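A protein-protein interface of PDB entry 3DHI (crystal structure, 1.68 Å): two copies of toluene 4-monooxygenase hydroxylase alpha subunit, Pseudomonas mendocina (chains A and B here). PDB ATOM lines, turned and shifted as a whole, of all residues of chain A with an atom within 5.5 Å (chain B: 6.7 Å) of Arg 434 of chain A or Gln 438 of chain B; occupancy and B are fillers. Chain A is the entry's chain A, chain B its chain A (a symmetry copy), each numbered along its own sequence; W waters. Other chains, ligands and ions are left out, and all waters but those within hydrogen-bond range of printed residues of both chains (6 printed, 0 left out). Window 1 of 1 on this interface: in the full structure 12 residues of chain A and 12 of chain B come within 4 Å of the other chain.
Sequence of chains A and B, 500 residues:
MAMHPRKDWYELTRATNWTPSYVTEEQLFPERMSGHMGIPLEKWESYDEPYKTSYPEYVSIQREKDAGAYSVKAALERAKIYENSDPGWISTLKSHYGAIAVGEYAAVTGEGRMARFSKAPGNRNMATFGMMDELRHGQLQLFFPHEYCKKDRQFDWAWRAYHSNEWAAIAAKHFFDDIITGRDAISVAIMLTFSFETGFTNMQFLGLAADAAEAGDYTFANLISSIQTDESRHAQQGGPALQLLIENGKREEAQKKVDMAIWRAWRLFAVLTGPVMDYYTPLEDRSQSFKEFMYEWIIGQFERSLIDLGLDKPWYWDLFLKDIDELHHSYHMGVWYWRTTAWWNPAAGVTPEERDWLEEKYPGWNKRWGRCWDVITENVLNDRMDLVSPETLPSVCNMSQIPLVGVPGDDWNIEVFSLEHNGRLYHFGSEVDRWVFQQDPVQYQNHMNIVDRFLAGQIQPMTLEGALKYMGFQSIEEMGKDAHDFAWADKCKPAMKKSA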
ATOM      1  N   PHE A 417       9.463 -14.075   8.237  1.00  0.00           N
ATOM      2  CA  PHE A 417       8.461 -14.494   7.262  1.00  0.00           C
ATOM      3  C   PHE A 417       9.186 -14.645   5.940  1.00  0.00           C
ATOM      4  O   PHE A 417       9.564 -13.656   5.327  1.00  0.00           O
ATOM      5  CB  PHE A 417       7.344 -13.445   7.216  1.00  0.00           C
ATOM      6  CG  PHE A 417       6.616 -13.327   8.513  1.00  0.00           C
ATOM      7  CD1 PHE A 417       5.494 -14.093   8.749  1.00  0.00           C
ATOM      8  CD2 PHE A 417       7.103 -12.502   9.548  1.00  0.00           C
ATOM      9  CE1 PHE A 417       4.829 -14.023   9.982  1.00  0.00           C
ATOM     10  CE2 PHE A 417       6.443 -12.418  10.771  1.00  0.00           C
ATOM     11  CZ  PHE A 417       5.304 -13.179  10.991  1.00  0.00           C
ATOM     12  N   SER A 418       9.411 -15.891   5.519  1.00  0.00           N
ATOM     13  CA  SER A 418      10.279 -16.124   4.372  1.00  0.00           C
ATOM     14  C   SER A 418       9.465 -16.373   3.108  1.00  0.00           C
ATOM     15  O   SER A 418       8.267 -16.648   3.173  1.00  0.00           O
ATOM     16  CB  SER A 418      11.258 -17.277   4.622  1.00  0.00           C
ATOM     17  OG  SER A 418      12.153 -16.944   5.672  1.00  0.00           O
ATOM     18  N   LEU A 419      10.125 -16.238   1.968  1.00  0.00           N
ATOM     19  CA  LEU A 419       9.485 -16.383   0.672  1.00  0.00           C
ATOM     20  C   LEU A 419      10.474 -16.827  -0.398  1.00  0.00           C
ATOM     21  O   LEU A 419      11.536 -16.229  -0.560  1.00  0.00           O
ATOM     22  CB  LEU A 419       8.866 -15.040   0.226  1.00  0.00           C
ATOM     23  CG  LEU A 419       8.087 -15.005  -1.102  1.00  0.00           C
ATOM     24  CD1 LEU A 419       6.788 -15.779  -1.012  1.00  0.00           C
ATOM     25  CD2 LEU A 419       7.803 -13.582  -1.529  1.00  0.00           C
ATOM     26  N   PHE A 428      11.533 -11.605   5.424  1.00  0.00           N
ATOM     27  CA  PHE A 428      10.827 -10.384   5.827  1.00  0.00           C
ATOM     28  C   PHE A 428      10.570 -10.317   7.323  1.00  0.00           C
ATOM     29  O   PHE A 428      10.387 -11.357   8.002  1.00  0.00           O
ATOM     30  CB  PHE A 428       9.505 -10.273   5.037  1.00  0.00           C
ATOM     31  CG  PHE A 428       9.708 -10.285   3.557  1.00  0.00           C
ATOM     32  CD1 PHE A 428      10.109  -9.123   2.890  1.00  0.00           C
ATOM     33  CD2 PHE A 428       9.551 -11.472   2.822  1.00  0.00           C
ATOM     34  CE1 PHE A 428      10.337  -9.114   1.508  1.00  0.00           C
ATOM     35  CE2 PHE A 428       9.768 -11.470   1.413  1.00  0.00           C
ATOM     36  CZ  PHE A 428      10.171 -10.299   0.768  1.00  0.00           C
ATOM     37  N   SER A 430       7.932  -9.102   8.880  1.00  0.00           N
ATOM     38  CA  SER A 430       6.524  -9.180   9.272  1.00  0.00           C
ATOM     39  C   SER A 430       5.737  -9.795   8.130  1.00  0.00           C
ATOM     40  O   SER A 430       6.234  -9.883   6.995  1.00  0.00           O
ATOM     41  CB  SER A 430       5.953  -7.791   9.574  1.00  0.00           C
ATOM     42  OG  SER A 430       5.902  -7.034   8.361  1.00  0.00           O
ATOM     43  N   GLU A 431       4.512 -10.217   8.442  1.00  0.00           N
ATOM     44  CA  GLU A 431       3.582 -10.724   7.439  1.00  0.00           C
ATOM     45  C   GLU A 431       3.322  -9.623   6.413  1.00  0.00           C
ATOM     46  O   GLU A 431       3.123  -9.891   5.205  1.00  0.00           O
ATOM     47  CB  GLU A 431       2.245 -11.059   8.112  1.00  0.00           C
ATOM     48  CG  GLU A 431       2.212 -12.377   8.843  1.00  0.00           C
ATOM     49  CD  GLU A 431       2.116 -13.594   7.921  1.00  0.00           C
ATOM     50  OE1 GLU A 431       2.022 -14.703   8.478  1.00  0.00           O
ATOM     51  OE2 GLU A 431       2.131 -13.447   6.668  1.00  0.00           O
ATOM     52  N   VAL A 432       3.283  -8.385   6.909  1.00  0.00           N
ATOM     53  CA  VAL A 432       2.890  -7.276   6.047  1.00  0.00           C
ATOM     54  C   VAL A 432       4.011  -6.985   5.047  1.00  0.00           C
ATOM     55  O   VAL A 432       3.764  -6.712   3.872  1.00  0.00           O
ATOM     56  CB  VAL A 432       2.564  -5.984   6.843  1.00  0.00           C
ATOM     57  CG1 VAL A 432       1.853  -4.990   5.941  1.00  0.00           C
ATOM     58  CG2 VAL A 432       1.687  -6.257   8.076  1.00  0.00           C
ATOM     59  N   ASP A 433       5.262  -7.034   5.505  1.00  0.00           N
ATOM     60  CA  ASP A 433       6.374  -6.794   4.569  1.00  0.00           C
ATOM     61  C   ASP A 433       6.404  -7.821   3.435  1.00  0.00           C
ATOM     62  O   ASP A 433       6.618  -7.488   2.253  1.00  0.00           O
ATOM     63  CB  ASP A 433       7.718  -6.733   5.321  1.00  0.00           C
ATOM     64  CG  ASP A 433       7.868  -5.442   6.095  1.00  0.00           C
ATOM     65  OD1 ASP A 433       7.979  -4.385   5.436  1.00  0.00           O
ATOM     66  OD2 ASP A 433       7.797  -5.471   7.332  1.00  0.00           O
ATOM     67  N   ARG A 434       6.179  -9.083   3.793  1.00  0.00           N
ATOM     68  CA  ARG A 434       6.097 -10.139   2.784  1.00  0.00           C
ATOM     69  C   ARG A 434       4.940  -9.872   1.822  1.00  0.00           C
ATOM     70  O   ARG A 434       5.090 -10.025   0.614  1.00  0.00           O
ATOM     71  CB  ARG A 434       5.944 -11.502   3.454  1.00  0.00           C
ATOM     72  CG  ARG A 434       5.978 -12.646   2.444  1.00  0.00           C
ATOM     73  CD  ARG A 434       6.096 -14.029   3.154  1.00  0.00           C
ATOM     74  NE  ARG A 434       4.975 -14.308   4.052  1.00  0.00           N
ATOM     75  CZ  ARG A 434       4.922 -15.353   4.877  1.00  0.00           C
ATOM     76  NH1 ARG A 434       5.929 -16.225   4.905  1.00  0.00           N
ATOM     77  NH2 ARG A 434       3.871 -15.530   5.673  1.00  0.00           N
ATOM     78  N   TRP A 435       3.802  -9.443   2.369  1.00  0.00           N
ATOM     79  CA  TRP A 435       2.610  -9.127   1.563  1.00  0.00           C
ATOM     80  C   TRP A 435       2.910  -7.980   0.583  1.00  0.00           C
ATOM     81  O   TRP A 435       2.562  -8.062  -0.591  1.00  0.00           O
ATOM     82  CB  TRP A 435       1.446  -8.793   2.512  1.00  0.00           C
ATOM     83  CG  TRP A 435       0.198  -8.281   1.832  1.00  0.00           C
ATOM     84  CD1 TRP A 435      -0.780  -9.037   1.226  1.00  0.00           C
ATOM     85  CD2 TRP A 435      -0.200  -6.925   1.695  1.00  0.00           C
ATOM     86  NE1 TRP A 435      -1.770  -8.214   0.729  1.00  0.00           N
ATOM     87  CE2 TRP A 435      -1.430  -6.914   0.992  1.00  0.00           C
ATOM     88  CE3 TRP A 435       0.368  -5.705   2.077  1.00  0.00           C
ATOM     89  CZ2 TRP A 435      -2.104  -5.726   0.678  1.00  0.00           C
ATOM     90  CZ3 TRP A 435      -0.312  -4.523   1.767  1.00  0.00           C
ATOM     91  CH2 TRP A 435      -1.531  -4.545   1.075  1.00  0.00           C
ATOM     92  N   VAL A 436       3.603  -6.935   1.048  1.00  0.00           N
ATOM     93  CA  VAL A 436       3.972  -5.823   0.161  1.00  0.00           C
ATOM     94  C   VAL A 436       4.781  -6.320  -1.069  1.00  0.00           C
ATOM     95  O   VAL A 436       4.542  -5.916  -2.214  1.00  0.00           O
ATOM     96  CB  VAL A 436       4.784  -4.775   0.951  1.00  0.00           C
ATOM     97  CG1 VAL A 436       5.427  -3.750  -0.011  1.00  0.00           C
ATOM     98  CG2 VAL A 436       3.913  -4.070   2.007  1.00  0.00           C
ATOM     99  N   PHE A 437       5.757  -7.193  -0.813  1.00  0.00           N
ATOM    100  CA  PHE A 437       6.581  -7.752  -1.886  1.00  0.00           C
ATOM    101  C   PHE A 437       5.697  -8.472  -2.907  1.00  0.00           C
ATOM    102  O   PHE A 437       5.852  -8.302  -4.113  1.00  0.00           O
ATOM    103  CB  PHE A 437       7.597  -8.736  -1.282  1.00  0.00           C
ATOM    104  CG  PHE A 437       8.531  -9.345  -2.281  1.00  0.00           C
ATOM    105  CD1 PHE A 437       9.822  -8.837  -2.428  1.00  0.00           C
ATOM    106  CD2 PHE A 437       8.149 -10.446  -3.039  1.00  0.00           C
ATOM    107  CE1 PHE A 437      10.713  -9.392  -3.332  1.00  0.00           C
ATOM    108  CE2 PHE A 437       9.039 -11.030  -3.942  1.00  0.00           C
ATOM    109  CZ  PHE A 437      10.325 -10.493  -4.091  1.00  0.00           C
ATOM    110  N   GLN A 438       4.771  -9.276  -2.401  1.00  0.00           N
ATOM    111  CA  GLN A 438       3.911 -10.085  -3.270  1.00  0.00           C
ATOM    112  C   GLN A 438       2.926  -9.242  -4.077  1.00  0.00           C
ATOM    113  O   GLN A 438       2.422  -9.697  -5.109  1.00  0.00           O
ATOM    114  CB  GLN A 438       3.188 -11.140  -2.448  1.00  0.00           C
ATOM    115  CG  GLN A 438       4.153 -12.182  -1.888  1.00  0.00           C
ATOM    116  CD  GLN A 438       3.469 -13.121  -0.931  1.00  0.00           C
ATOM    117  OE1 GLN A 438       3.000 -12.714   0.138  1.00  0.00           O
ATOM    118  NE2 GLN A 438       3.397 -14.394  -1.313  1.00  0.00           N
ATOM    119  N   GLN A 439       2.656  -8.021  -3.617  1.00  0.00           N
ATOM    120  CA  GLN A 439       1.766  -7.126  -4.363  1.00  0.00           C
ATOM    121  C   GLN A 439       2.392  -6.632  -5.652  1.00  0.00           C
ATOM    122  O   GLN A 439       1.678  -6.304  -6.598  1.00  0.00           O
ATOM    123  CB  GLN A 439       1.333  -5.922  -3.519  1.00  0.00           C
ATOM    124  CG  GLN A 439       0.550  -6.287  -2.262  1.00  0.00           C
ATOM    125  CD  GLN A 439      -0.442  -7.416  -2.498  1.00  0.00           C
ATOM    126  OE1 GLN A 439      -1.438  -7.245  -3.208  1.00  0.00           O
ATOM    127  NE2 GLN A 439      -0.163  -8.591  -1.917  1.00  0.00           N
ATOM    128  N   MET B 399      -5.402 -24.738  -1.684  1.00  0.00           N
ATOM    129  CA  MET B 399      -5.880 -24.888  -0.292  1.00  0.00           C
ATOM    130  C   MET B 399      -7.297 -25.435  -0.258  1.00  0.00           C
ATOM    131  O   MET B 399      -7.519 -26.554   0.203  1.00  0.00           O
ATOM    132  CB  MET B 399      -5.763 -23.561   0.481  1.00  0.00           C
ATOM    133  CG  MET B 399      -6.156 -23.651   1.949  1.00  0.00           C
ATOM    134  SD  MET B 399      -5.227 -24.867   2.905  1.00  0.00           S
ATOM    135  CE  MET B 399      -3.533 -24.356   2.583  1.00  0.00           C
ATOM    136  N   LEU B 419       2.287 -18.897  -5.289  1.00  0.00           N
ATOM    137  CA  LEU B 419       3.378 -19.102  -4.351  1.00  0.00           C
ATOM    138  C   LEU B 419       4.342 -20.176  -4.836  1.00  0.00           C
ATOM    139  O   LEU B 419       3.931 -21.277  -5.191  1.00  0.00           O
ATOM    140  CB  LEU B 419       2.827 -19.537  -2.975  1.00  0.00           C
ATOM    141  CG  LEU B 419       3.830 -19.745  -1.826  1.00  0.00           C
ATOM    142  CD1 LEU B 419       4.441 -18.438  -1.368  1.00  0.00           C
ATOM    143  CD2 LEU B 419       3.176 -20.439  -0.652  1.00  0.00           C
ATOM    144  N   PHE B 428      -3.539 -20.099  -5.229  1.00  0.00           N
ATOM    145  CA  PHE B 428      -4.600 -19.948  -4.227  1.00  0.00           C
ATOM    146  C   PHE B 428      -5.683 -18.974  -4.656  1.00  0.00           C
ATOM    147  O   PHE B 428      -5.426 -17.993  -5.396  1.00  0.00           O
ATOM    148  CB  PHE B 428      -3.975 -19.518  -2.883  1.00  0.00           C
ATOM    149  CG  PHE B 428      -2.936 -20.471  -2.392  1.00  0.00           C
ATOM    150  CD1 PHE B 428      -3.310 -21.654  -1.745  1.00  0.00           C
ATOM    151  CD2 PHE B 428      -1.571 -20.222  -2.617  1.00  0.00           C
ATOM    152  CE1 PHE B 428      -2.356 -22.580  -1.303  1.00  0.00           C
ATOM    153  CE2 PHE B 428      -0.593 -21.151  -2.159  1.00  0.00           C
ATOM    154  CZ  PHE B 428      -0.989 -22.327  -1.519  1.00  0.00           C
ATOM    155  N   GLU B 431      -5.910 -14.194  -0.775  1.00  0.00           N
ATOM    156  CA  GLU B 431      -4.746 -13.869   0.041  1.00  0.00           C
ATOM    157  C   GLU B 431      -4.753 -14.762   1.280  1.00  0.00           C
ATOM    158  O   GLU B 431      -3.687 -15.168   1.797  1.00  0.00           O
ATOM    159  CB  GLU B 431      -4.851 -12.414   0.516  1.00  0.00           C
ATOM    160  CG  GLU B 431      -4.452 -11.379  -0.506  1.00  0.00           C
ATOM    161  CD  GLU B 431      -2.941 -11.263  -0.711  1.00  0.00           C
ATOM    162  OE1 GLU B 431      -2.557 -10.378  -1.498  1.00  0.00           O
ATOM    163  OE2 GLU B 431      -2.152 -12.032  -0.096  1.00  0.00           O
ATOM    164  N   ASP B 433      -6.111 -17.804   1.724  1.00  0.00           N
ATOM    165  CA  ASP B 433      -5.728 -19.204   1.471  1.00  0.00           C
ATOM    166  C   ASP B 433      -4.211 -19.379   1.374  1.00  0.00           C
ATOM    167  O   ASP B 433      -3.624 -20.334   1.918  1.00  0.00           O
ATOM    168  CB  ASP B 433      -6.448 -19.750   0.222  1.00  0.00           C
ATOM    169  CG  ASP B 433      -7.911 -20.021   0.494  1.00  0.00           C
ATOM    170  OD1 ASP B 433      -8.188 -20.950   1.284  1.00  0.00           O
ATOM    171  OD2 ASP B 433      -8.764 -19.275  -0.009  1.00  0.00           O
ATOM    172  N   ARG B 434      -3.565 -18.442   0.682  1.00  0.00           N
ATOM    173  CA  ARG B 434      -2.105 -18.458   0.594  1.00  0.00           C
ATOM    174  C   ARG B 434      -1.484 -18.309   1.983  1.00  0.00           C
ATOM    175  O   ARG B 434      -0.533 -19.010   2.315  1.00  0.00           O
ATOM    176  CB  ARG B 434      -1.620 -17.354  -0.341  1.00  0.00           C
ATOM    177  CG  ARG B 434      -0.109 -17.407  -0.559  1.00  0.00           C
ATOM    178  CD  ARG B 434       0.334 -16.460  -1.716  1.00  0.00           C
ATOM    179  NE  ARG B 434       0.007 -15.057  -1.462  1.00  0.00           N
ATOM    180  CZ  ARG B 434       0.151 -14.083  -2.359  1.00  0.00           C
ATOM    181  NH1 ARG B 434       0.630 -14.365  -3.569  1.00  0.00           N
ATOM    182  NH2 ARG B 434      -0.182 -12.832  -2.054  1.00  0.00           N
ATOM    183  N   TRP B 435      -2.051 -17.414   2.792  1.00  0.00           N
ATOM    184  CA  TRP B 435      -1.571 -17.176   4.165  1.00  0.00           C
ATOM    185  C   TRP B 435      -1.702 -18.455   5.010  1.00  0.00           C
ATOM    186  O   TRP B 435      -0.772 -18.823   5.722  1.00  0.00           O
ATOM    187  CB  TRP B 435      -2.355 -15.997   4.766  1.00  0.00           C
ATOM    188  CG  TRP B 435      -2.095 -15.743   6.232  1.00  0.00           C
ATOM    189  CD1 TRP B 435      -1.036 -15.049   6.773  1.00  0.00           C
ATOM    190  CD2 TRP B 435      -2.897 -16.166   7.324  1.00  0.00           C
ATOM    191  NE1 TRP B 435      -1.149 -15.016   8.148  1.00  0.00           N
ATOM    192  CE2 TRP B 435      -2.275 -15.706   8.510  1.00  0.00           C
ATOM    193  CE3 TRP B 435      -4.077 -16.912   7.428  1.00  0.00           C
ATOM    194  CZ2 TRP B 435      -2.805 -15.957   9.783  1.00  0.00           C
ATOM    195  CZ3 TRP B 435      -4.605 -17.155   8.700  1.00  0.00           C
ATOM    196  CH2 TRP B 435      -3.969 -16.680   9.855  1.00  0.00           C
ATOM    197  N   VAL B 436      -2.832 -19.161   4.893  1.00  0.00           N
ATOM    198  CA  VAL B 436      -3.012 -20.419   5.629  1.00  0.00           C
ATOM    199  C   VAL B 436      -1.877 -21.431   5.313  1.00  0.00           C
ATOM    200  O   VAL B 436      -1.318 -22.085   6.203  1.00  0.00           O
ATOM    201  CB  VAL B 436      -4.388 -21.029   5.288  1.00  0.00           C
ATOM    202  CG1 VAL B 436      -4.483 -22.479   5.814  1.00  0.00           C
ATOM    203  CG2 VAL B 436      -5.537 -20.165   5.839  1.00  0.00           C
ATOM    204  N   PHE B 437      -1.555 -21.566   4.024  1.00  0.00           N
ATOM    205  CA  PHE B 437      -0.490 -22.473   3.594  1.00  0.00           C
ATOM    206  C   PHE B 437       0.830 -22.093   4.269  1.00  0.00           C
ATOM    207  O   PHE B 437       1.554 -22.944   4.775  1.00  0.00           O
ATOM    208  CB  PHE B 437      -0.343 -22.392   2.066  1.00  0.00           C
ATOM    209  CG  PHE B 437       0.691 -23.313   1.498  1.00  0.00           C
ATOM    210  CD1 PHE B 437       0.306 -24.525   0.924  1.00  0.00           C
ATOM    211  CD2 PHE B 437       2.035 -22.960   1.490  1.00  0.00           C
ATOM    212  CE1 PHE B 437       1.241 -25.387   0.375  1.00  0.00           C
ATOM    213  CE2 PHE B 437       2.990 -23.807   0.925  1.00  0.00           C
ATOM    214  CZ  PHE B 437       2.587 -25.030   0.372  1.00  0.00           C
ATOM    215  N   GLN B 438       1.125 -20.800   4.264  1.00  0.00           N
ATOM    216  CA  GLN B 438       2.396 -20.310   4.805  1.00  0.00           C
ATOM    217  C   GLN B 438       2.489 -20.460   6.322  1.00  0.00           C
ATOM    218  O   GLN B 438       3.593 -20.470   6.878  1.00  0.00           O
ATOM    219  CB  GLN B 438       2.620 -18.867   4.380  1.00  0.00           C
ATOM    220  CG  GLN B 438       2.843 -18.748   2.875  1.00  0.00           C
ATOM    221  CD  GLN B 438       2.887 -17.312   2.428  1.00  0.00           C
ATOM    222  OE1 GLN B 438       1.894 -16.582   2.523  1.00  0.00           O
ATOM    223  NE2 GLN B 438       4.051 -16.886   1.941  1.00  0.00           N
ATOM    224  N   GLN B 439       1.343 -20.580   6.990  1.00  0.00           N
ATOM    225  CA  GLN B 439       1.345 -20.787   8.441  1.00  0.00           C
ATOM    226  C   GLN B 439       1.853 -22.161   8.829  1.00  0.00           C
ATOM    227  O   GLN B 439       2.375 -22.339   9.929  1.00  0.00           O
ATOM    228  CB  GLN B 439      -0.046 -20.575   9.049  1.00  0.00           C
ATOM    229  CG  GLN B 439      -0.604 -19.167   8.859  1.00  0.00           C
ATOM    230  CD  GLN B 439       0.452 -18.089   9.044  1.00  0.00           C
ATOM    231  OE1 GLN B 439       0.945 -17.867  10.155  1.00  0.00           O
ATOM    232  NE2 GLN B 439       0.826 -17.421   7.943  1.00  0.00           N
ATOM    233  N   ASP B 440       1.665 -23.147   7.949  1.00  0.00           N
ATOM    234  CA  ASP B 440       2.014 -24.532   8.304  1.00  0.00           C
ATOM    235  C   ASP B 440       2.333 -25.365   7.044  1.00  0.00           C
ATOM    236  O   ASP B 440       1.602 -26.296   6.698  1.00  0.00           O
ATOM    237  CB  ASP B 440       0.847 -25.129   9.109  1.00  0.00           C
ATOM    238  CG  ASP B 440       1.196 -26.452   9.790  1.00  0.00           C
ATOM    239  OD1 ASP B 440       2.394 -26.817   9.898  1.00  0.00           O
ATOM    240  OD2 ASP B 440       0.255 -27.129  10.240  1.00  0.00           O
ATOM    241  N   PRO B 441       3.417 -25.023   6.329  1.00  0.00           N
ATOM    242  CA  PRO B 441       3.650 -25.687   5.037  1.00  0.00           C
ATOM    243  C   PRO B 441       3.789 -27.209   5.116  1.00  0.00           C
ATOM    244  O   PRO B 441       3.418 -27.908   4.176  1.00  0.00           O
ATOM    245  CB  PRO B 441       4.966 -25.070   4.535  1.00  0.00           C
ATOM    246  CG  PRO B 441       5.196 -23.871   5.369  1.00  0.00           C
ATOM    247  CD  PRO B 441       4.410 -23.973   6.628  1.00  0.00           C
ATOM    248  N   TYR B 444       0.722 -29.200   4.241  1.00  0.00           N
ATOM    249  CA  TYR B 444       0.130 -29.053   2.907  1.00  0.00           C
ATOM    250  C   TYR B 444       1.083 -29.294   1.740  1.00  0.00           C
ATOM    251  O   TYR B 444       0.629 -29.561   0.624  1.00  0.00           O
ATOM    252  CB  TYR B 444      -0.420 -27.619   2.706  1.00  0.00           C
ATOM    253  CG  TYR B 444      -1.284 -27.100   3.817  1.00  0.00           C
ATOM    254  CD1 TYR B 444      -0.810 -26.118   4.702  1.00  0.00           C
ATOM    255  CD2 TYR B 444      -2.555 -27.628   4.033  1.00  0.00           C
ATOM    256  CE1 TYR B 444      -1.600 -25.650   5.757  1.00  0.00           C
ATOM    257  CE2 TYR B 444      -3.355 -27.170   5.072  1.00  0.00           C
ATOM    258  CZ  TYR B 444      -2.877 -26.180   5.936  1.00  0.00           C
ATOM    259  OH  TYR B 444      -3.681 -25.742   6.946  1.00  0.00           O
HETATM  260  O   HOH W   1       6.374 -18.494   1.850  1.00  0.00           O
HETATM  261  O   HOH W   2       4.835 -17.923   7.319  1.00  0.00           O
HETATM  262  O   HOH W   3       1.498 -13.911   2.085  1.00  0.00           O
HETATM  263  O   HOH W   4       1.334 -14.987  11.065  1.00  0.00           O
HETATM  264  O   HOH W   5       0.207 -11.489  -4.777  1.00  0.00           O
HETATM  265  O   HOH W   6      -4.127  -8.339  -2.287  1.00  0.00           O
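OE1 of Gln 438 of chain B sits close to O of Arg 434 of chain B, at 3.4 Å.
The side-chain carboxylate of Glu 431 of chain B is in salt-bridge range of the guanidinium group of Arg 434 of chain B (2.9 Å).
O of Ser 418 of chain A sits at hydrogen-bond distance from NH1 of Arg 434 of chain A, 2.9 Å away.
OE2 of Glu 431 of chain A is in salt-bridge range of NH2 of Arg 434 of chain A (2.9 Å).
The backbone carbonyl oxygen (O) of Trp 435 of chain B is in hydrogen-bond range of the side-chain amide nitrogen (NE2) of Gln 439 of chain B (3.1 Å).
The backbone carbonyl oxygen (O) of Trp 435 of chain A sits at hydrogen-bond distance from the side-chain amide nitrogen (NE2) of Gln 439 of chain A (3.1 Å).
Arg 434 of chain A touches just one residue of chain B: Gln 438 (3.4 Å).
Of the printed residues of chain A, Gln 438 of chain B touches Arg 434.
Of the printed residues of chain B, Glu 431 of chain A touches Trp 435 (3.2 Å) and Gln 439 (3.0 Å).
Printed residues of chain B within 4 Å of Gln 439 of chain A: Glu 431.
Asp 433 of chain A touches none of the printed residues of chain B.
Pro 441 of chain B touches none of the printed residues of chain A.
The nearest residue of chain B that does not touch Arg 434 of chain A is Gln 439 of chain B (4.2 Å).
The nearest printed residue of chain A that does not touch Arg 434 of chain B is Gln 439 of chain A (4.2 Å).
Hydrophobic or aromatic side chains of chain A that line the printed part of chain B: Leu 419 and Trp 435.
Of the 14 printed residues of chain B, 6 touch a printed residue of chain A.
Along chain B the printed residues that touch a printed residue of chain A span positions 419 to 439.
Among the printed residues, 7 pairs touch across the chains.
Among the printed residues, no Asp or Glu carboxylate lies within 4 Å of a Lys or Arg side-chain nitrogen of the other chain.
Water W4 bridges OE1 of Glu 431 of chain A (2.7 Å) and OE1 of Gln 439 of chain B (3.0 Å).
Water W6 bridges OE1 of Glu 431 of chain B (2.7 Å) and OE1 of Gln 439 of chain A (3.0 Å).
Water W3 bridges OE1 of Gln 438 of chain B (2.7 Å) and OE1 of Gln 438 of chain A (2.7 Å).
Water W1 bridges the side-chain amide nitrogen (NE2) of Gln 438 of chain B (2.8 Å) and the backbone carbonyl oxygen (O) of Ser 418 of chain A (3.0 Å).
Water W2 lies within hydrogen-bond range of the backbone carbonyl oxygen of Gln 438 of chain B (2.9 Å) and the guanidinium group of Arg 434 of chain A (3.1 Å).
Water W5 bridges the backbone carbonyl oxygen (O) of Gln 438 of chain A and the guanidinium group (NH2) of Arg 434 of chain B.
OE1 of Glu 431 of chain A is in hydrogen-bond range of NE2 of Gln 439 of chain B, at 3.0 Å.
The side-chain amide nitrogen (NE2) of Gln 438 of chain A sits close to the guanidinium group (NE) of Arg 434 of chain B, at 3.5 Å.
NE1 of Trp 435 of chain A is in hydrogen-bond range of OE1 of Glu 431 of chain B.
NE of Arg 434 of chain A sits close to NE2 of Gln 438 of chain B (3.5 Å).
The side-chain carboxylate of Glu 431 of chain A is in hydrogen-bond range of the indole nitrogen of Trp 435 of chain B (3.2 Å).
NE2 of Gln 439 of chain A is in hydrogen-bond range of OE1 of Glu 431 of chain B (3.0 Å).
Leu 419 of chain A touches Leu 419 of chain B.
Leu 419 of chain A touches its own counterpart, Leu 419 of chain B.
Glu 431 of chain A touches Trp 435 of chain B, and with the chains exchanged Trp 435 of chain A touches Glu 431 of chain B.
Glu 431 of chain A touches Gln 439 of chain B, and with the chains exchanged Gln 439 of chain A touches Glu 431 of chain B.
Arg 434 of chain A touches Gln 438 of chain B, and with the chains exchanged Gln 438 of chain A touches Arg 434 of chain B.
Positions printed for both chains: 419, 428, 431, 433, 434, 435, 436, 437, 438 and 439.
Of the 7 pairs that touch across the chains among the printed residues, 7 have their exchanged pair printed and touching as well.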
